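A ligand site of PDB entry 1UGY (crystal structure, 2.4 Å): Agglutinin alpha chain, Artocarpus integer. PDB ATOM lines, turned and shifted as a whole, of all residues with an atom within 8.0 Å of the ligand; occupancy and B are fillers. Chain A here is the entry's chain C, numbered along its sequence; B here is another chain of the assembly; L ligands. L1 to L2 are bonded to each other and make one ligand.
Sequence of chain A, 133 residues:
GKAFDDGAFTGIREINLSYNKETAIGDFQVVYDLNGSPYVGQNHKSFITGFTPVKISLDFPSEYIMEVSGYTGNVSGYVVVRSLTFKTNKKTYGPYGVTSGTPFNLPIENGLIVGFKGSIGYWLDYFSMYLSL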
ATOM      1  N   GLY A   1      -9.723  10.551 -26.285  1.00  0.00           N
ATOM      2  CA  GLY A   1      -8.538   9.738 -25.917  1.00  0.00           C
ATOM      3  C   GLY A   1      -8.521   8.405 -26.619  1.00  0.00           C
ATOM      4  O   GLY A   1      -9.294   8.156 -27.542  1.00  0.00           O
ATOM      5  N   LYS A   2      -7.628   7.522 -26.166  1.00  0.00           N
ATOM      6  CA  LYS A   2      -7.475   6.190 -26.727  1.00  0.00           C
ATOM      7  C   LYS A   2      -8.323   5.204 -25.912  1.00  0.00           C
ATOM      8  O   LYS A   2      -8.059   4.992 -24.727  1.00  0.00           O
ATOM      9  CB  LYS A   2      -6.006   5.786 -26.681  1.00  0.00           C
ATOM     10  CG  LYS A   2      -5.661   4.507 -27.382  1.00  0.00           C
ATOM     11  CD  LYS A   2      -4.177   4.225 -27.239  1.00  0.00           C
ATOM     12  CE  LYS A   2      -3.656   3.250 -28.298  1.00  0.00           C
ATOM     13  NZ  LYS A   2      -4.347   1.931 -28.230  1.00  0.00           N
ATOM     14  N   ALA A  24      -6.237  15.153 -12.539  1.00  0.00           N
ATOM     15  CA  ALA A  24      -7.092  13.975 -12.469  1.00  0.00           C
ATOM     16  C   ALA A  24      -6.330  12.663 -12.520  1.00  0.00           C
ATOM     17  O   ALA A  24      -5.100  12.639 -12.412  1.00  0.00           O
ATOM     18  CB  ALA A  24      -8.110  14.024 -13.583  1.00  0.00           C
ATOM     19  N   ILE A  25      -7.071  11.576 -12.700  1.00  0.00           N
ATOM     20  CA  ILE A  25      -6.501  10.233 -12.780  1.00  0.00           C
ATOM     21  C   ILE A  25      -5.823  10.068 -14.145  1.00  0.00           C
ATOM     22  O   ILE A  25      -6.374  10.460 -15.180  1.00  0.00           O
ATOM     23  CB  ILE A  25      -7.622   9.162 -12.622  1.00  0.00           C
ATOM     24  CG1 ILE A  25      -8.345   9.336 -11.283  1.00  0.00           C
ATOM     25  CG2 ILE A  25      -7.025   7.771 -12.742  1.00  0.00           C
ATOM     26  CD1 ILE A  25      -7.475   9.131 -10.046  1.00  0.00           C
ATOM     27  N   SER A  46      -1.327   7.524 -19.778  1.00  0.00           N
ATOM     28  CA  SER A  46      -1.661   8.891 -20.160  1.00  0.00           C
ATOM     29  C   SER A  46      -0.729   9.349 -21.298  1.00  0.00           C
ATOM     30  O   SER A  46       0.361   8.802 -21.463  1.00  0.00           O
ATOM     31  CB  SER A  46      -1.467   9.795 -18.937  1.00  0.00           C
ATOM     32  OG  SER A  46      -1.497  11.164 -19.283  1.00  0.00           O
ATOM     33  N   PHE A  47      -1.163  10.340 -22.077  1.00  0.00           N
ATOM     34  CA  PHE A  47      -0.342  10.871 -23.176  1.00  0.00           C
ATOM     35  C   PHE A  47       0.796  11.703 -22.608  1.00  0.00           C
ATOM     36  O   PHE A  47       1.774  11.990 -23.297  1.00  0.00           O
ATOM     37  CB  PHE A  47      -1.152  11.763 -24.121  1.00  0.00           C
ATOM     38  CG  PHE A  47      -2.208  11.044 -24.923  1.00  0.00           C
ATOM     39  CD1 PHE A  47      -2.164   9.659 -25.077  1.00  0.00           C
ATOM     40  CD2 PHE A  47      -3.228  11.755 -25.541  1.00  0.00           C
ATOM     41  CE1 PHE A  47      -3.138   8.998 -25.847  1.00  0.00           C
ATOM     42  CE2 PHE A  47      -4.192  11.114 -26.309  1.00  0.00           C
ATOM     43  CZ  PHE A  47      -4.148   9.729 -26.463  1.00  0.00           C
ATOM     44  N   ILE A  48       0.663  12.117 -21.345  1.00  0.00           N
ATOM     45  CA  ILE A  48       1.692  12.921 -20.681  1.00  0.00           C
ATOM     46  C   ILE A  48       2.164  12.235 -19.407  1.00  0.00           C
ATOM     47  O   ILE A  48       1.665  11.179 -19.045  1.00  0.00           O
ATOM     48  CB  ILE A  48       1.164  14.330 -20.312  1.00  0.00           C
ATOM     49  CG1 ILE A  48      -0.084  14.215 -19.425  1.00  0.00           C
ATOM     50  CG2 ILE A  48       0.839  15.105 -21.576  1.00  0.00           C
ATOM     51  CD1 ILE A  48      -0.521  15.517 -18.814  1.00  0.00           C
ATOM     52  N   VAL A  75     -11.586  19.541 -16.760  1.00  0.00           N
ATOM     53  CA  VAL A  75     -10.174  19.865 -16.629  1.00  0.00           C
ATOM     54  C   VAL A  75      -9.712  20.343 -17.989  1.00  0.00           C
ATOM     55  O   VAL A  75      -9.780  19.593 -18.968  1.00  0.00           O
ATOM     56  CB  VAL A  75      -9.361  18.649 -16.185  1.00  0.00           C
ATOM     57  CG1 VAL A  75      -7.878  18.955 -16.265  1.00  0.00           C
ATOM     58  CG2 VAL A  75      -9.719  18.279 -14.758  1.00  0.00           C
ATOM     59  N   SER A  76      -9.271  21.591 -18.056  1.00  0.00           N
ATOM     60  CA  SER A  76      -8.812  22.197 -19.296  1.00  0.00           C
ATOM     61  C   SER A  76      -9.768  22.009 -20.469  1.00  0.00           C
ATOM     62  O   SER A  76      -9.354  21.832 -21.601  1.00  0.00           O
ATOM     63  CB  SER A  76      -7.437  21.652 -19.687  1.00  0.00           C
ATOM     64  OG  SER A  76      -6.451  22.068 -18.749  1.00  0.00           O
ATOM     65  N   GLY A  77     -11.066  22.042 -20.185  1.00  0.00           N
ATOM     66  CA  GLY A  77     -12.056  21.893 -21.238  1.00  0.00           C
ATOM     67  C   GLY A  77     -12.573  20.495 -21.500  1.00  0.00           C
ATOM     68  O   GLY A  77     -13.401  20.312 -22.388  1.00  0.00           O
ATOM     69  N   TYR A  78     -12.113  19.503 -20.742  1.00  0.00           N
ATOM     70  CA  TYR A  78     -12.558  18.124 -20.936  1.00  0.00           C
ATOM     71  C   TYR A  78     -13.168  17.546 -19.669  1.00  0.00           C
ATOM     72  O   TYR A  78     -12.690  17.808 -18.569  1.00  0.00           O
ATOM     73  CB  TYR A  78     -11.372  17.239 -21.359  1.00  0.00           C
ATOM     74  CG  TYR A  78     -10.716  17.615 -22.667  1.00  0.00           C
ATOM     75  CD1 TYR A  78     -11.299  17.282 -23.891  1.00  0.00           C
ATOM     76  CD2 TYR A  78      -9.524  18.350 -22.675  1.00  0.00           C
ATOM     77  CE1 TYR A  78     -10.712  17.661 -25.102  1.00  0.00           C
ATOM     78  CE2 TYR A  78      -8.935  18.743 -23.884  1.00  0.00           C
ATOM     79  CZ  TYR A  78      -9.531  18.393 -25.079  1.00  0.00           C
ATOM     80  OH  TYR A  78      -8.941  18.783 -26.269  1.00  0.00           O
ATOM     81  N   VAL A  79     -14.231  16.767 -19.821  1.00  0.00           N
ATOM     82  CA  VAL A  79     -14.860  16.121 -18.673  1.00  0.00           C
ATOM     83  C   VAL A  79     -14.087  14.818 -18.470  1.00  0.00           C
ATOM     84  O   VAL A  79     -14.021  13.978 -19.372  1.00  0.00           O
ATOM     85  CB  VAL A  79     -16.349  15.785 -18.920  1.00  0.00           C
ATOM     86  CG1 VAL A  79     -16.916  14.979 -17.759  1.00  0.00           C
ATOM     87  CG2 VAL A  79     -17.148  17.070 -19.073  1.00  0.00           C
ATOM     88  N   VAL A  80     -13.482  14.660 -17.296  1.00  0.00           N
ATOM     89  CA  VAL A  80     -12.715  13.473 -16.986  1.00  0.00           C
ATOM     90  C   VAL A  80     -12.979  12.987 -15.573  1.00  0.00           C
ATOM     91  O   VAL A  80     -13.622  13.672 -14.777  1.00  0.00           O
ATOM     92  CB  VAL A  80     -11.198  13.756 -17.133  1.00  0.00           C
ATOM     93  CG1 VAL A  80     -10.881  14.145 -18.564  1.00  0.00           C
ATOM     94  CG2 VAL A  80     -10.786  14.861 -16.164  1.00  0.00           C
ATOM     95  N   VAL A  81     -12.484  11.788 -15.252  1.00  0.00           N
ATOM     96  CA  VAL A  81     -12.648  11.242 -13.917  1.00  0.00           C
ATOM     97  C   VAL A  81     -11.537  11.842 -13.075  1.00  0.00           C
ATOM     98  O   VAL A  81     -10.362  11.493 -13.240  1.00  0.00           O
ATOM     99  CB  VAL A  81     -12.513   9.704 -13.917  1.00  0.00           C
ATOM    100  CG1 VAL A  81     -12.695   9.178 -12.496  1.00  0.00           C
ATOM    101  CG2 VAL A  81     -13.534   9.092 -14.859  1.00  0.00           C
ATOM    102  N   SER A 119     -11.446   4.954 -21.607  1.00  0.00           N
ATOM    103  CA  SER A 119     -10.665   5.755 -22.534  1.00  0.00           C
ATOM    104  C   SER A 119      -9.727   6.653 -21.738  1.00  0.00           C
ATOM    105  O   SER A 119     -10.104   7.174 -20.683  1.00  0.00           O
ATOM    106  CB  SER A 119     -11.603   6.595 -23.404  1.00  0.00           C
ATOM    107  OG  SER A 119     -10.887   7.585 -24.116  1.00  0.00           O
ATOM    108  N   ILE A 120      -8.506   6.822 -22.230  1.00  0.00           N
ATOM    109  CA  ILE A 120      -7.509   7.651 -21.560  1.00  0.00           C
ATOM    110  C   ILE A 120      -6.764   8.516 -22.566  1.00  0.00           C
ATOM    111  O   ILE A 120      -6.182   8.008 -23.514  1.00  0.00           O
ATOM    112  CB  ILE A 120      -6.491   6.776 -20.782  1.00  0.00           C
ATOM    113  CG1 ILE A 120      -7.216   5.964 -19.700  1.00  0.00           C
ATOM    114  CG2 ILE A 120      -5.427   7.650 -20.132  1.00  0.00           C
ATOM    115  CD1 ILE A 120      -6.334   4.926 -19.035  1.00  0.00           C
ATOM    116  N   GLY A 121      -6.803   9.829 -22.351  1.00  0.00           N
ATOM    117  CA  GLY A 121      -6.094  10.766 -23.213  1.00  0.00           C
ATOM    118  C   GLY A 121      -5.030  11.341 -22.309  1.00  0.00           C
ATOM    119  O   GLY A 121      -4.072  10.654 -21.987  1.00  0.00           O
ATOM    120  N   TYR A 122      -5.171  12.599 -21.912  1.00  0.00           N
ATOM    121  CA  TYR A 122      -4.212  13.161 -20.971  1.00  0.00           C
ATOM    122  C   TYR A 122      -4.638  12.559 -19.622  1.00  0.00           C
ATOM    123  O   TYR A 122      -3.807  12.223 -18.784  1.00  0.00           O
ATOM    124  CB  TYR A 122      -4.292  14.692 -20.906  1.00  0.00           C
ATOM    125  CG  TYR A 122      -3.430  15.395 -21.933  1.00  0.00           C
ATOM    126  CD1 TYR A 122      -3.078  16.730 -21.758  1.00  0.00           C
ATOM    127  CD2 TYR A 122      -2.962  14.730 -23.066  1.00  0.00           C
ATOM    128  CE1 TYR A 122      -2.261  17.390 -22.687  1.00  0.00           C
ATOM    129  CE2 TYR A 122      -2.147  15.376 -23.996  1.00  0.00           C
ATOM    130  CZ  TYR A 122      -1.806  16.710 -23.800  1.00  0.00           C
ATOM    131  OH  TYR A 122      -0.975  17.350 -24.692  1.00  0.00           O
ATOM    132  N   TRP A 123      -5.952  12.406 -19.443  1.00  0.00           N
ATOM    133  CA  TRP A 123      -6.514  11.849 -18.218  1.00  0.00           C
ATOM    134  C   TRP A 123      -7.565  10.804 -18.548  1.00  0.00           C
ATOM    135  O   TRP A 123      -7.920  10.615 -19.710  1.00  0.00           O
ATOM    136  CB  TRP A 123      -7.135  12.957 -17.376  1.00  0.00           C
ATOM    137  CG  TRP A 123      -6.171  14.067 -17.130  1.00  0.00           C
ATOM    138  CD1 TRP A 123      -5.104  14.046 -16.279  1.00  0.00           C
ATOM    139  CD2 TRP A 123      -6.130  15.325 -17.801  1.00  0.00           C
ATOM    140  NE1 TRP A 123      -4.383  15.217 -16.400  1.00  0.00           N
ATOM    141  CE2 TRP A 123      -4.995  16.020 -17.333  1.00  0.00           C
ATOM    142  CE3 TRP A 123      -6.945  15.935 -18.774  1.00  0.00           C
ATOM    143  CZ2 TRP A 123      -4.639  17.291 -17.784  1.00  0.00           C
ATOM    144  CZ3 TRP A 123      -6.597  17.201 -19.236  1.00  0.00           C
ATOM    145  CH2 TRP A 123      -5.450  17.862 -18.743  1.00  0.00           C
ATOM    146  N   LEU A 124      -8.074  10.123 -17.517  1.00  0.00           N
ATOM    147  CA  LEU A 124      -9.105   9.111 -17.682  1.00  0.00           C
ATOM    148  C   LEU A 124     -10.417   9.780 -18.090  1.00  0.00           C
ATOM    149  O   LEU A 124     -11.076  10.422 -17.279  1.00  0.00           O
ATOM    150  CB  LEU A 124      -9.282   8.339 -16.366  1.00  0.00           C
ATOM    151  CG  LEU A 124     -10.329   7.227 -16.292  1.00  0.00           C
ATOM    152  CD1 LEU A 124     -10.040   6.142 -17.336  1.00  0.00           C
ATOM    153  CD2 LEU A 124     -10.334   6.639 -14.883  1.00  0.00           C
ATOM    154  N   ASP A 125     -10.778   9.634 -19.366  1.00  0.00           N
ATOM    155  CA  ASP A 125     -11.993  10.250 -19.901  1.00  0.00           C
ATOM    156  C   ASP A 125     -13.283   9.684 -19.325  1.00  0.00           C
ATOM    157  O   ASP A 125     -14.208  10.437 -19.014  1.00  0.00           O
ATOM    158  CB  ASP A 125     -12.014  10.103 -21.428  1.00  0.00           C
ATOM    159  CG  ASP A 125     -10.773  10.685 -22.088  1.00  0.00           C
ATOM    160  OD1 ASP A 125     -10.421  11.841 -21.796  1.00  0.00           O
ATOM    161  OD2 ASP A 125     -10.158   9.971 -22.916  1.00  0.00           O
ATOM    162  N   TYR A 126     -13.340   8.368 -19.198  1.00  0.00           N
ATOM    163  CA  TYR A 126     -14.512   7.687 -18.669  1.00  0.00           C
ATOM    164  C   TYR A 126     -14.209   6.207 -18.553  1.00  0.00           C
ATOM    165  O   TYR A 126     -13.221   5.721 -19.097  1.00  0.00           O
ATOM    166  CB  TYR A 126     -15.705   7.887 -19.626  1.00  0.00           C
ATOM    167  CG  TYR A 126     -15.496   7.285 -21.003  1.00  0.00           C
ATOM    168  CD1 TYR A 126     -15.577   5.913 -21.205  1.00  0.00           C
ATOM    169  CD2 TYR A 126     -15.231   8.098 -22.108  1.00  0.00           C
ATOM    170  CE1 TYR A 126     -15.388   5.363 -22.472  1.00  0.00           C
ATOM    171  CE2 TYR A 126     -15.041   7.563 -23.382  1.00  0.00           C
ATOM    172  CZ  TYR A 126     -15.119   6.188 -23.555  1.00  0.00           C
ATOM    173  OH  TYR A 126     -14.949   5.646 -24.808  1.00  0.00           O
ATOM    174  N   ALA B  17     -16.694  11.646 -19.240  1.00  0.00           N
ATOM    175  CA  ALA B  17     -17.067  12.255 -20.512  1.00  0.00           C
ATOM    176  C   ALA B  17     -18.170  11.464 -21.209  1.00  0.00           C
ATOM    177  O   ALA B  17     -18.370  10.275 -20.931  1.00  0.00           O
ATOM    178  CB  ALA B  17     -15.852  12.348 -21.420  1.00  0.00           C
HETATM  179  C1  LIG L   1      -3.467  16.370 -27.498  1.00  0.00           C
HETATM  180  C2  LIG L   1      -4.028  17.337 -28.534  1.00  0.00           C
HETATM  181  C3  LIG L   1      -4.641  18.603 -27.924  1.00  0.00           C
HETATM  182  C4  LIG L   1      -5.443  18.333 -26.690  1.00  0.00           C
HETATM  183  C5  LIG L   1      -4.673  17.442 -25.722  1.00  0.00           C
HETATM  184  C6  LIG L   1      -5.549  17.028 -24.582  1.00  0.00           C
HETATM  185  O1  LIG L   1      -2.252  16.869 -27.094  1.00  0.00           O
HETATM  186  O2  LIG L   1      -2.896  17.738 -29.301  1.00  0.00           O
HETATM  187  O3  LIG L   1      -5.528  19.173 -28.856  1.00  0.00           O
HETATM  188  O4  LIG L   1      -5.737  19.583 -26.088  1.00  0.00           O
HETATM  189  O5  LIG L   1      -4.295  16.200 -26.349  1.00  0.00           O
HETATM  190  O6  LIG L   1      -6.618  16.204 -25.114  1.00  0.00           O
HETATM  191  C1  LG2 L   2      -6.525  14.824 -24.846  1.00  0.00           C
HETATM  192  C2  LG2 L   2      -7.289  13.971 -25.883  1.00  0.00           C
HETATM  193  C3  LG2 L   2      -8.798  14.145 -25.724  1.00  0.00           C
HETATM  194  C4  LG2 L   2      -9.180  13.757 -24.298  1.00  0.00           C
HETATM  195  C5  LG2 L   2      -8.390  14.626 -23.301  1.00  0.00           C
HETATM  196  C6  LG2 L   2      -8.703  14.312 -21.840  1.00  0.00           C
HETATM  197  O1  LG2 L   2      -6.903  14.302 -27.206  1.00  0.00           O
HETATM  198  O2  LG2 L   2      -9.491  13.345 -26.679  1.00  0.00           O
HETATM  199  O3  LG2 L   2      -8.965  12.370 -24.092  1.00  0.00           O
HETATM  200  O4  LG2 L   2      -6.953  14.497 -23.519  1.00  0.00           O
HETATM  201  O5  LG2 L   2      -7.989  13.172 -21.398  1.00  0.00           O
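The backbone NH of Tyr 122 sits at hydrogen-bond distance from an oxygen (O5) of LG2 L2, at 2.9 Å. N of Gly 1 is in hydrogen-bond range of O2 of LG2 L2, 2.8 Å away. O of Trp 123 is in hydrogen-bond range of O5 of LG2 L2. The backbone NH of Trp 123 is in hydrogen-bond range of an oxygen (O5) of LG2 L2, 2.9 Å away. The side-chain hydroxyl (OH) of Tyr 78 lies within hydrogen-bond range of an oxygen (O4) of LIG L1 (3.3 Å). OH of Tyr 122 sits at hydrogen-bond distance from O1 of LIG L1. OD1 of Asp 125 sits at hydrogen-bond distance from O3 of LG2 L2 (2.8 Å).
The backbone NH of Gly 121 sits at hydrogen-bond distance from the side-chain carboxylate of Asp 125, 3.4 Å away. The side-chain carboxylate (OD2) of Asp 125 sits at hydrogen-bond distance from the side-chain hydroxyl (OG) of Ser 119, 2.8 Å away. The backbone NH of Ala 17 of chain B is in hydrogen-bond range of the backbone carbonyl oxygen of Asp 125 (2.8 Å). The backbone carbonyl oxygen (O) of Tyr 122 is in hydrogen-bond range of the side-chain hydroxyl (OG) of Ser 46 (2.6 Å). N of Phe 47 sits at hydrogen-bond distance from O of Gly 121 (2.9 Å). The backbone NH (N) of Gly 1 sits close to the side-chain carboxylate (OD2) of Asp 125 (3.4 Å).
CG1 of Val 80 touches C6 of LG2 L2, at 3.9 Å. CA of Gly 121 touches O3 of LG2 L2, at 3.4 Å. Hydrophobic or aromatic side chains that line the ligand: Tyr 78, Val 80, Tyr 122 and Trp 123. Of the 23 residues printed, 7 come within 4 Å of the ligand. The nearest printed residue that does not touch the ligand is Phe 47 (4.2 Å).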
